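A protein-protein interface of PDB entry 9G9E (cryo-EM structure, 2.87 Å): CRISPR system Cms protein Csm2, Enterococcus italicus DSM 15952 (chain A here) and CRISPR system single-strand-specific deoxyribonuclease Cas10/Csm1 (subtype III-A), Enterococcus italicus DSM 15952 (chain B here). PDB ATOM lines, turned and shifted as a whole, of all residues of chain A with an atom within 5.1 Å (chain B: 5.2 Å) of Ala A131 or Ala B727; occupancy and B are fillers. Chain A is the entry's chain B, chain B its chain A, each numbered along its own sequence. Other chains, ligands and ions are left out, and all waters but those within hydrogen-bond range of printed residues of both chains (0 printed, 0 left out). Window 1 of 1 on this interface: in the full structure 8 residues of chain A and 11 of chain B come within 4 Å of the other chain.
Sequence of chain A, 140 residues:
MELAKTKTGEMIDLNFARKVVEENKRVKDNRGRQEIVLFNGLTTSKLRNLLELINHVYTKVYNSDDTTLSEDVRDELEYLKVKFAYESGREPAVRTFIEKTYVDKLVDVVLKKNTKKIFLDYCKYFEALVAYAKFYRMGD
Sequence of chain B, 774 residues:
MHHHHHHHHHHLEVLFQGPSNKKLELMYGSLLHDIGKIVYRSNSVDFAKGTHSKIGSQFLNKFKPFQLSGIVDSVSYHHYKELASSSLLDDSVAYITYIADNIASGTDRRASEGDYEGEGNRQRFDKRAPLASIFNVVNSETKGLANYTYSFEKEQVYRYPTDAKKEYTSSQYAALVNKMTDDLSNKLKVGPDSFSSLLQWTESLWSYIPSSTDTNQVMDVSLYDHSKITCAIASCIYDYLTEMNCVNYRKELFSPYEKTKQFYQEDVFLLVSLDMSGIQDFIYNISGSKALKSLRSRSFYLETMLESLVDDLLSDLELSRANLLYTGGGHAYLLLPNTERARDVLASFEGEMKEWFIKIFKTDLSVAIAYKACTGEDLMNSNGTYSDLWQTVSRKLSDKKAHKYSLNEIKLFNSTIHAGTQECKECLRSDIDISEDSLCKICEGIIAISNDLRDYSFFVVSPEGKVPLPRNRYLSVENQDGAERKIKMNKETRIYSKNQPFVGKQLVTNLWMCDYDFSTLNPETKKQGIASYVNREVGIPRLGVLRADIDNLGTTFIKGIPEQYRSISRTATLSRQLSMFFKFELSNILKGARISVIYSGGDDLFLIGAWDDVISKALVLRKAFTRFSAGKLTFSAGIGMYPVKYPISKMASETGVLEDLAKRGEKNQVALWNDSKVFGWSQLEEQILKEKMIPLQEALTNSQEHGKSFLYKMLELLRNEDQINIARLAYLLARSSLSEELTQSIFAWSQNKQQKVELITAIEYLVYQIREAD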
ATOM      1  N   PHE A 126     -33.679 -10.346  -3.318  1.00  0.00           N
ATOM      2  CA  PHE A 126     -33.890  -9.162  -2.487  1.00  0.00           C
ATOM      3  C   PHE A 126     -32.788  -8.130  -2.704  1.00  0.00           C
ATOM      4  O   PHE A 126     -33.059  -6.923  -2.777  1.00  0.00           O
ATOM      5  CB  PHE A 126     -33.967  -9.567  -1.014  1.00  0.00           C
ATOM      6  CG  PHE A 126     -34.803  -8.643  -0.175  1.00  0.00           C
ATOM      7  CD1 PHE A 126     -34.249  -7.508   0.391  1.00  0.00           C
ATOM      8  CD2 PHE A 126     -36.142  -8.912   0.051  1.00  0.00           C
ATOM      9  CE1 PHE A 126     -35.016  -6.658   1.164  1.00  0.00           C
ATOM     10  CE2 PHE A 126     -36.914  -8.067   0.823  1.00  0.00           C
ATOM     11  CZ  PHE A 126     -36.350  -6.938   1.380  1.00  0.00           C
ATOM     12  N   GLU A 127     -31.538  -8.587  -2.806  1.00  0.00           N
ATOM     13  CA  GLU A 127     -30.426  -7.668  -3.027  1.00  0.00           C
ATOM     14  C   GLU A 127     -30.543  -6.975  -4.378  1.00  0.00           C
ATOM     15  O   GLU A 127     -30.300  -5.768  -4.487  1.00  0.00           O
ATOM     16  CB  GLU A 127     -29.100  -8.419  -2.917  1.00  0.00           C
ATOM     17  CG  GLU A 127     -27.892  -7.620  -3.365  1.00  0.00           C
ATOM     18  CD  GLU A 127     -26.634  -8.459  -3.434  1.00  0.00           C
ATOM     19  OE1 GLU A 127     -26.710  -9.674  -3.151  1.00  0.00           O
ATOM     20  OE2 GLU A 127     -25.566  -7.902  -3.761  1.00  0.00           O
ATOM     21  N   ALA A 128     -30.916  -7.723  -5.420  1.00  0.00           N
ATOM     22  CA  ALA A 128     -31.128  -7.122  -6.732  1.00  0.00           C
ATOM     23  C   ALA A 128     -32.285  -6.133  -6.698  1.00  0.00           C
ATOM     24  O   ALA A 128     -32.231  -5.078  -7.340  1.00  0.00           O
ATOM     25  CB  ALA A 128     -31.386  -8.212  -7.772  1.00  0.00           C
ATOM     26  N   LEU A 129     -33.343  -6.466  -5.959  1.00  0.00           N
ATOM     27  CA  LEU A 129     -34.469  -5.556  -5.790  1.00  0.00           C
ATOM     28  C   LEU A 129     -34.013  -4.231  -5.196  1.00  0.00           C
ATOM     29  O   LEU A 129     -34.336  -3.155  -5.714  1.00  0.00           O
ATOM     30  CB  LEU A 129     -35.510  -6.217  -4.891  1.00  0.00           C
ATOM     31  CG  LEU A 129     -36.874  -6.593  -5.455  1.00  0.00           C
ATOM     32  CD1 LEU A 129     -37.697  -7.189  -4.337  1.00  0.00           C
ATOM     33  CD2 LEU A 129     -37.567  -5.383  -6.052  1.00  0.00           C
ATOM     34  N   VAL A 130     -33.245  -4.297  -4.106  1.00  0.00           N
ATOM     35  CA  VAL A 130     -32.770  -3.080  -3.450  1.00  0.00           C
ATOM     36  C   VAL A 130     -31.829  -2.309  -4.370  1.00  0.00           C
ATOM     37  O   VAL A 130     -31.878  -1.074  -4.441  1.00  0.00           O
ATOM     38  CB  VAL A 130     -32.099  -3.426  -2.109  1.00  0.00           C
ATOM     39  CG1 VAL A 130     -31.515  -2.178  -1.465  1.00  0.00           C
ATOM     40  CG2 VAL A 130     -33.099  -4.090  -1.179  1.00  0.00           C
ATOM     41  N   ALA A 131     -30.960  -3.025  -5.088  1.00  0.00           N
ATOM     42  CA  ALA A 131     -30.013  -2.371  -5.984  1.00  0.00           C
ATOM     43  C   ALA A 131     -30.733  -1.619  -7.096  1.00  0.00           C
ATOM     44  O   ALA A 131     -30.408  -0.464  -7.390  1.00  0.00           O
ATOM     45  CB  ALA A 131     -29.052  -3.406  -6.568  1.00  0.00           C
ATOM     46  N   TYR A 132     -31.728  -2.256  -7.719  1.00  0.00           N
ATOM     47  CA  TYR A 132     -32.483  -1.588  -8.773  1.00  0.00           C
ATOM     48  C   TYR A 132     -33.290  -0.419  -8.219  1.00  0.00           C
ATOM     49  O   TYR A 132     -33.371   0.642  -8.853  1.00  0.00           O
ATOM     50  CB  TYR A 132     -33.396  -2.587  -9.483  1.00  0.00           C
ATOM     51  CG  TYR A 132     -32.658  -3.583 -10.351  1.00  0.00           C
ATOM     52  CD1 TYR A 132     -31.644  -3.172 -11.207  1.00  0.00           C
ATOM     53  CD2 TYR A 132     -32.980  -4.933 -10.320  1.00  0.00           C
ATOM     54  CE1 TYR A 132     -30.969  -4.079 -12.002  1.00  0.00           C
ATOM     55  CE2 TYR A 132     -32.309  -5.846 -11.111  1.00  0.00           C
ATOM     56  CZ  TYR A 132     -31.306  -5.415 -11.949  1.00  0.00           C
ATOM     57  OH  TYR A 132     -30.638  -6.323 -12.739  1.00  0.00           O
ATOM     58  N   ALA A 133     -33.883  -0.588  -7.034  1.00  0.00           N
ATOM     59  CA  ALA A 133     -34.635   0.504  -6.426  1.00  0.00           C
ATOM     60  C   ALA A 133     -33.742   1.713  -6.184  1.00  0.00           C
ATOM     61  O   ALA A 133     -34.150   2.853  -6.428  1.00  0.00           O
ATOM     62  CB  ALA A 133     -35.281   0.039  -5.122  1.00  0.00           C
ATOM     63  N   LYS A 134     -32.517   1.481  -5.708  1.00  0.00           N
ATOM     64  CA  LYS A 134     -31.568   2.580  -5.553  1.00  0.00           C
ATOM     65  C   LYS A 134     -31.147   3.143  -6.906  1.00  0.00           C
ATOM     66  O   LYS A 134     -30.897   4.347  -7.033  1.00  0.00           O
ATOM     67  CB  LYS A 134     -30.347   2.111  -4.763  1.00  0.00           C
ATOM     68  CG  LYS A 134     -30.385   2.470  -3.288  1.00  0.00           C
ATOM     69  CD  LYS A 134     -30.236   3.968  -3.080  1.00  0.00           C
ATOM     70  CE  LYS A 134     -28.940   4.486  -3.681  1.00  0.00           C
ATOM     71  NZ  LYS A 134     -28.766   5.946  -3.451  1.00  0.00           N
ATOM     72  N   PHE A 135     -31.055   2.285  -7.926  1.00  0.00           N
ATOM     73  CA  PHE A 135     -30.603   2.734  -9.240  1.00  0.00           C
ATOM     74  C   PHE A 135     -31.601   3.688  -9.886  1.00  0.00           C
ATOM     75  O   PHE A 135     -31.201   4.684 -10.500  1.00  0.00           O
ATOM     76  CB  PHE A 135     -30.348   1.531 -10.147  1.00  0.00           C
ATOM     77  CG  PHE A 135     -29.784   1.895 -11.489  1.00  0.00           C
ATOM     78  CD1 PHE A 135     -28.611   2.627 -11.585  1.00  0.00           C
ATOM     79  CD2 PHE A 135     -30.424   1.509 -12.654  1.00  0.00           C
ATOM     80  CE1 PHE A 135     -28.088   2.967 -12.817  1.00  0.00           C
ATOM     81  CE2 PHE A 135     -29.906   1.846 -13.890  1.00  0.00           C
ATOM     82  CZ  PHE A 135     -28.737   2.576 -13.971  1.00  0.00           C
ATOM     83  N   GLN B 723     -25.989 -12.203 -13.481  1.00  0.00           N
ATOM     84  CA  GLN B 723     -27.106 -11.260 -13.448  1.00  0.00           C
ATOM     85  C   GLN B 723     -27.172 -10.524 -12.113  1.00  0.00           C
ATOM     86  O   GLN B 723     -27.414  -9.308 -12.069  1.00  0.00           O
ATOM     87  CB  GLN B 723     -28.416 -11.998 -13.720  1.00  0.00           C
ATOM     88  CG  GLN B 723     -29.655 -11.119 -13.692  1.00  0.00           C
ATOM     89  CD  GLN B 723     -29.705 -10.151 -14.856  1.00  0.00           C
ATOM     90  OE1 GLN B 723     -29.872 -10.554 -16.006  1.00  0.00           O
ATOM     91  NE2 GLN B 723     -29.558  -8.865 -14.562  1.00  0.00           N
ATOM     92  N   ILE B 724     -26.960 -11.246 -11.011  1.00  0.00           N
ATOM     93  CA  ILE B 724     -26.877 -10.591  -9.711  1.00  0.00           C
ATOM     94  C   ILE B 724     -25.726  -9.600  -9.705  1.00  0.00           C
ATOM     95  O   ILE B 724     -25.794  -8.556  -9.046  1.00  0.00           O
ATOM     96  CB  ILE B 724     -26.731 -11.632  -8.585  1.00  0.00           C
ATOM     97  CG1 ILE B 724     -27.557 -12.883  -8.892  1.00  0.00           C
ATOM     98  CG2 ILE B 724     -27.152 -11.031  -7.252  1.00  0.00           C
ATOM     99  CD1 ILE B 724     -29.051 -12.638  -8.947  1.00  0.00           C
ATOM    100  N   ASN B 725     -24.661  -9.893 -10.450  1.00  0.00           N
ATOM    101  CA  ASN B 725     -23.564  -8.940 -10.531  1.00  0.00           C
ATOM    102  C   ASN B 725     -23.940  -7.735 -11.386  1.00  0.00           C
ATOM    103  O   ASN B 725     -23.414  -6.640 -11.172  1.00  0.00           O
ATOM    104  CB  ASN B 725     -22.307  -9.622 -11.062  1.00  0.00           C
ATOM    105  CG  ASN B 725     -21.090  -9.289 -10.232  1.00  0.00           C
ATOM    106  OD1 ASN B 725     -21.134  -8.395  -9.391  1.00  0.00           O
ATOM    107  ND2 ASN B 725     -20.004 -10.015 -10.446  1.00  0.00           N
ATOM    108  N   ILE B 726     -24.857  -7.906 -12.343  1.00  0.00           N
ATOM    109  CA  ILE B 726     -25.443  -6.745 -13.009  1.00  0.00           C
ATOM    110  C   ILE B 726     -26.211  -5.893 -12.009  1.00  0.00           C
ATOM    111  O   ILE B 726     -26.194  -4.658 -12.077  1.00  0.00           O
ATOM    112  CB  ILE B 726     -26.341  -7.174 -14.184  1.00  0.00           C
ATOM    113  CG1 ILE B 726     -25.681  -8.281 -15.005  1.00  0.00           C
ATOM    114  CG2 ILE B 726     -26.690  -5.974 -15.042  1.00  0.00           C
ATOM    115  CD1 ILE B 726     -26.505  -8.724 -16.197  1.00  0.00           C
ATOM    116  N   ALA B 727     -26.913  -6.538 -11.074  1.00  0.00           N
ATOM    117  CA  ALA B 727     -27.577  -5.781 -10.016  1.00  0.00           C
ATOM    118  C   ALA B 727     -26.564  -5.023  -9.160  1.00  0.00           C
ATOM    119  O   ALA B 727     -26.790  -3.861  -8.793  1.00  0.00           O
ATOM    120  CB  ALA B 727     -28.422  -6.713  -9.152  1.00  0.00           C
ATOM    121  N   ARG B 728     -25.442  -5.668  -8.831  1.00  0.00           N
ATOM    122  CA  ARG B 728     -24.379  -4.981  -8.097  1.00  0.00           C
ATOM    123  C   ARG B 728     -23.844  -3.792  -8.887  1.00  0.00           C
ATOM    124  O   ARG B 728     -23.556  -2.735  -8.315  1.00  0.00           O
ATOM    125  CB  ARG B 728     -23.236  -5.944  -7.767  1.00  0.00           C
ATOM    126  CG  ARG B 728     -23.659  -7.316  -7.287  1.00  0.00           C
ATOM    127  CD  ARG B 728     -23.122  -7.617  -5.898  1.00  0.00           C
ATOM    128  NE  ARG B 728     -23.484  -8.957  -5.453  1.00  0.00           N
ATOM    129  CZ  ARG B 728     -22.959 -10.077  -5.933  1.00  0.00           C
ATOM    130  NH1 ARG B 728     -22.023 -10.059  -6.868  1.00  0.00           N
ATOM    131  NH2 ARG B 728     -23.381 -11.247  -5.461  1.00  0.00           N
ATOM    132  N   LEU B 729     -23.685  -3.956 -10.203  1.00  0.00           N
ATOM    133  CA  LEU B 729     -23.236  -2.855 -11.048  1.00  0.00           C
ATOM    134  C   LEU B 729     -24.234  -1.705 -11.032  1.00  0.00           C
ATOM    135  O   LEU B 729     -23.844  -0.533 -10.986  1.00  0.00           O
ATOM    136  CB  LEU B 729     -23.016  -3.348 -12.477  1.00  0.00           C
ATOM    137  CG  LEU B 729     -22.604  -2.290 -13.503  1.00  0.00           C
ATOM    138  CD1 LEU B 729     -21.256  -1.678 -13.146  1.00  0.00           C
ATOM    139  CD2 LEU B 729     -22.581  -2.883 -14.902  1.00  0.00           C
ATOM    140  N   ALA B 730     -25.529  -2.023 -11.084  1.00  0.00           N
ATOM    141  CA  ALA B 730     -26.550  -0.985 -11.008  1.00  0.00           C
ATOM    142  C   ALA B 730     -26.476  -0.242  -9.682  1.00  0.00           C
ATOM    143  O   ALA B 730     -26.585   0.990  -9.642  1.00  0.00           O
ATOM    144  CB  ALA B 730     -27.938  -1.594 -11.208  1.00  0.00           C
ATOM    145  N   TYR B 731     -26.284  -0.974  -8.582  1.00  0.00           N
ATOM    146  CA  TYR B 731     -26.156  -0.325  -7.279  1.00  0.00           C
ATOM    147  C   TYR B 731     -24.919   0.565  -7.222  1.00  0.00           C
ATOM    148  O   TYR B 731     -24.965   1.675  -6.675  1.00  0.00           O
ATOM    149  CB  TYR B 731     -26.112  -1.371  -6.167  1.00  0.00           C
ATOM    150  CG  TYR B 731     -26.163  -0.775  -4.779  1.00  0.00           C
ATOM    151  CD1 TYR B 731     -27.248  -0.009  -4.373  1.00  0.00           C
ATOM    152  CD2 TYR B 731     -25.127  -0.972  -3.877  1.00  0.00           C
ATOM    153  CE1 TYR B 731     -27.300   0.542  -3.107  1.00  0.00           C
ATOM    154  CE2 TYR B 731     -25.170  -0.426  -2.609  1.00  0.00           C
ATOM    155  CZ  TYR B 731     -26.258   0.330  -2.229  1.00  0.00           C
ATOM    156  OH  TYR B 731     -26.307   0.877  -0.967  1.00  0.00           O
ATOM    157  N   LEU B 732     -23.799   0.092  -7.777  1.00  0.00           N
ATOM    158  CA  LEU B 732     -22.587   0.902  -7.791  1.00  0.00           C
ATOM    159  C   LEU B 732     -22.788   2.173  -8.604  1.00  0.00           C
ATOM    160  O   LEU B 732     -22.362   3.256  -8.190  1.00  0.00           O
ATOM    161  CB  LEU B 732     -21.411   0.097  -8.346  1.00  0.00           C
ATOM    162  CG  LEU B 732     -20.160   0.922  -8.675  1.00  0.00           C
ATOM    163  CD1 LEU B 732     -19.640   1.640  -7.434  1.00  0.00           C
ATOM    164  CD2 LEU B 732     -19.072   0.066  -9.298  1.00  0.00           C
ATOM    165  N   ALA B 734     -25.610   3.677  -9.100  1.00  0.00           N
ATOM    166  CA  ALA B 734     -26.473   4.530  -8.290  1.00  0.00           C
ATOM    167  C   ALA B 734     -25.674   5.275  -7.229  1.00  0.00           C
ATOM    168  O   ALA B 734     -25.914   6.462  -6.979  1.00  0.00           O
ATOM    169  CB  ALA B 734     -27.573   3.694  -7.638  1.00  0.00           C
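The side-chain carboxylate of Glu A127 lies within salt-bridge range of the guanidinium group of Arg B728 (2.9 Å). The side-chain hydroxyl (OH) of Tyr A132 is in hydrogen-bond range of the side-chain amide nitrogen (NE2) of Gln B723, at 3.3 Å.
The guanidinium group of Arg B728 sits at hydrogen-bond distance from the side-chain amide oxygen of Asn B725 (3.2 Å).
Among the printed residues, merely in contact across the chains: Ala A131 with Ala B727 (3.2 Å), Phe A135 with Ala B730 (3.2 Å), Lys A134 with Ala B734 (3.4 Å), Phe A135 with Ala B734 (3.6 Å), Ala A128 with Ala B727 (3.6 Å), Ala A131 with Tyr B731 (3.6 Å), Lys A134 with Tyr B731 (3.6 Å) and Tyr A132 with Ala B730 (3.999 Å).
Of the printed residues of chain B, Ala A128 touches Ala B727. Of the printed residues of chain B, Ala A131 touches Ala B727 (3.2 Å) and Tyr B731 (3.6 Å). Of the printed residues of chain B, Tyr A132 touches Gln B723 and Ala B730. Of the printed residues of chain B, Phe A135 touches Ala B730 (3.2 Å) and Ala B734 (3.6 Å). Printed residues of chain A within 4 Å of Ala B727: Ala A128 and Ala A131. Leu B729 touches none of the printed residues of chain A. Leu B732 touches none of the printed residues of chain A. The nearest residue of chain A that does not touch Ala B727 is Tyr A132 (4.1 Å).
Printed residues of chain A that touch a printed residue of chain B: Glu A127, Ala A128, Ala A131, Tyr A132, Lys A134 and Phe A135. Among the printed residues, 10 pairs touch across the chains. Among the printed residues, Asp or Glu carboxylates within 4 Å of a Lys or Arg side-chain nitrogen of the other chain: Glu A127 with Arg B728 (2.9 Å).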
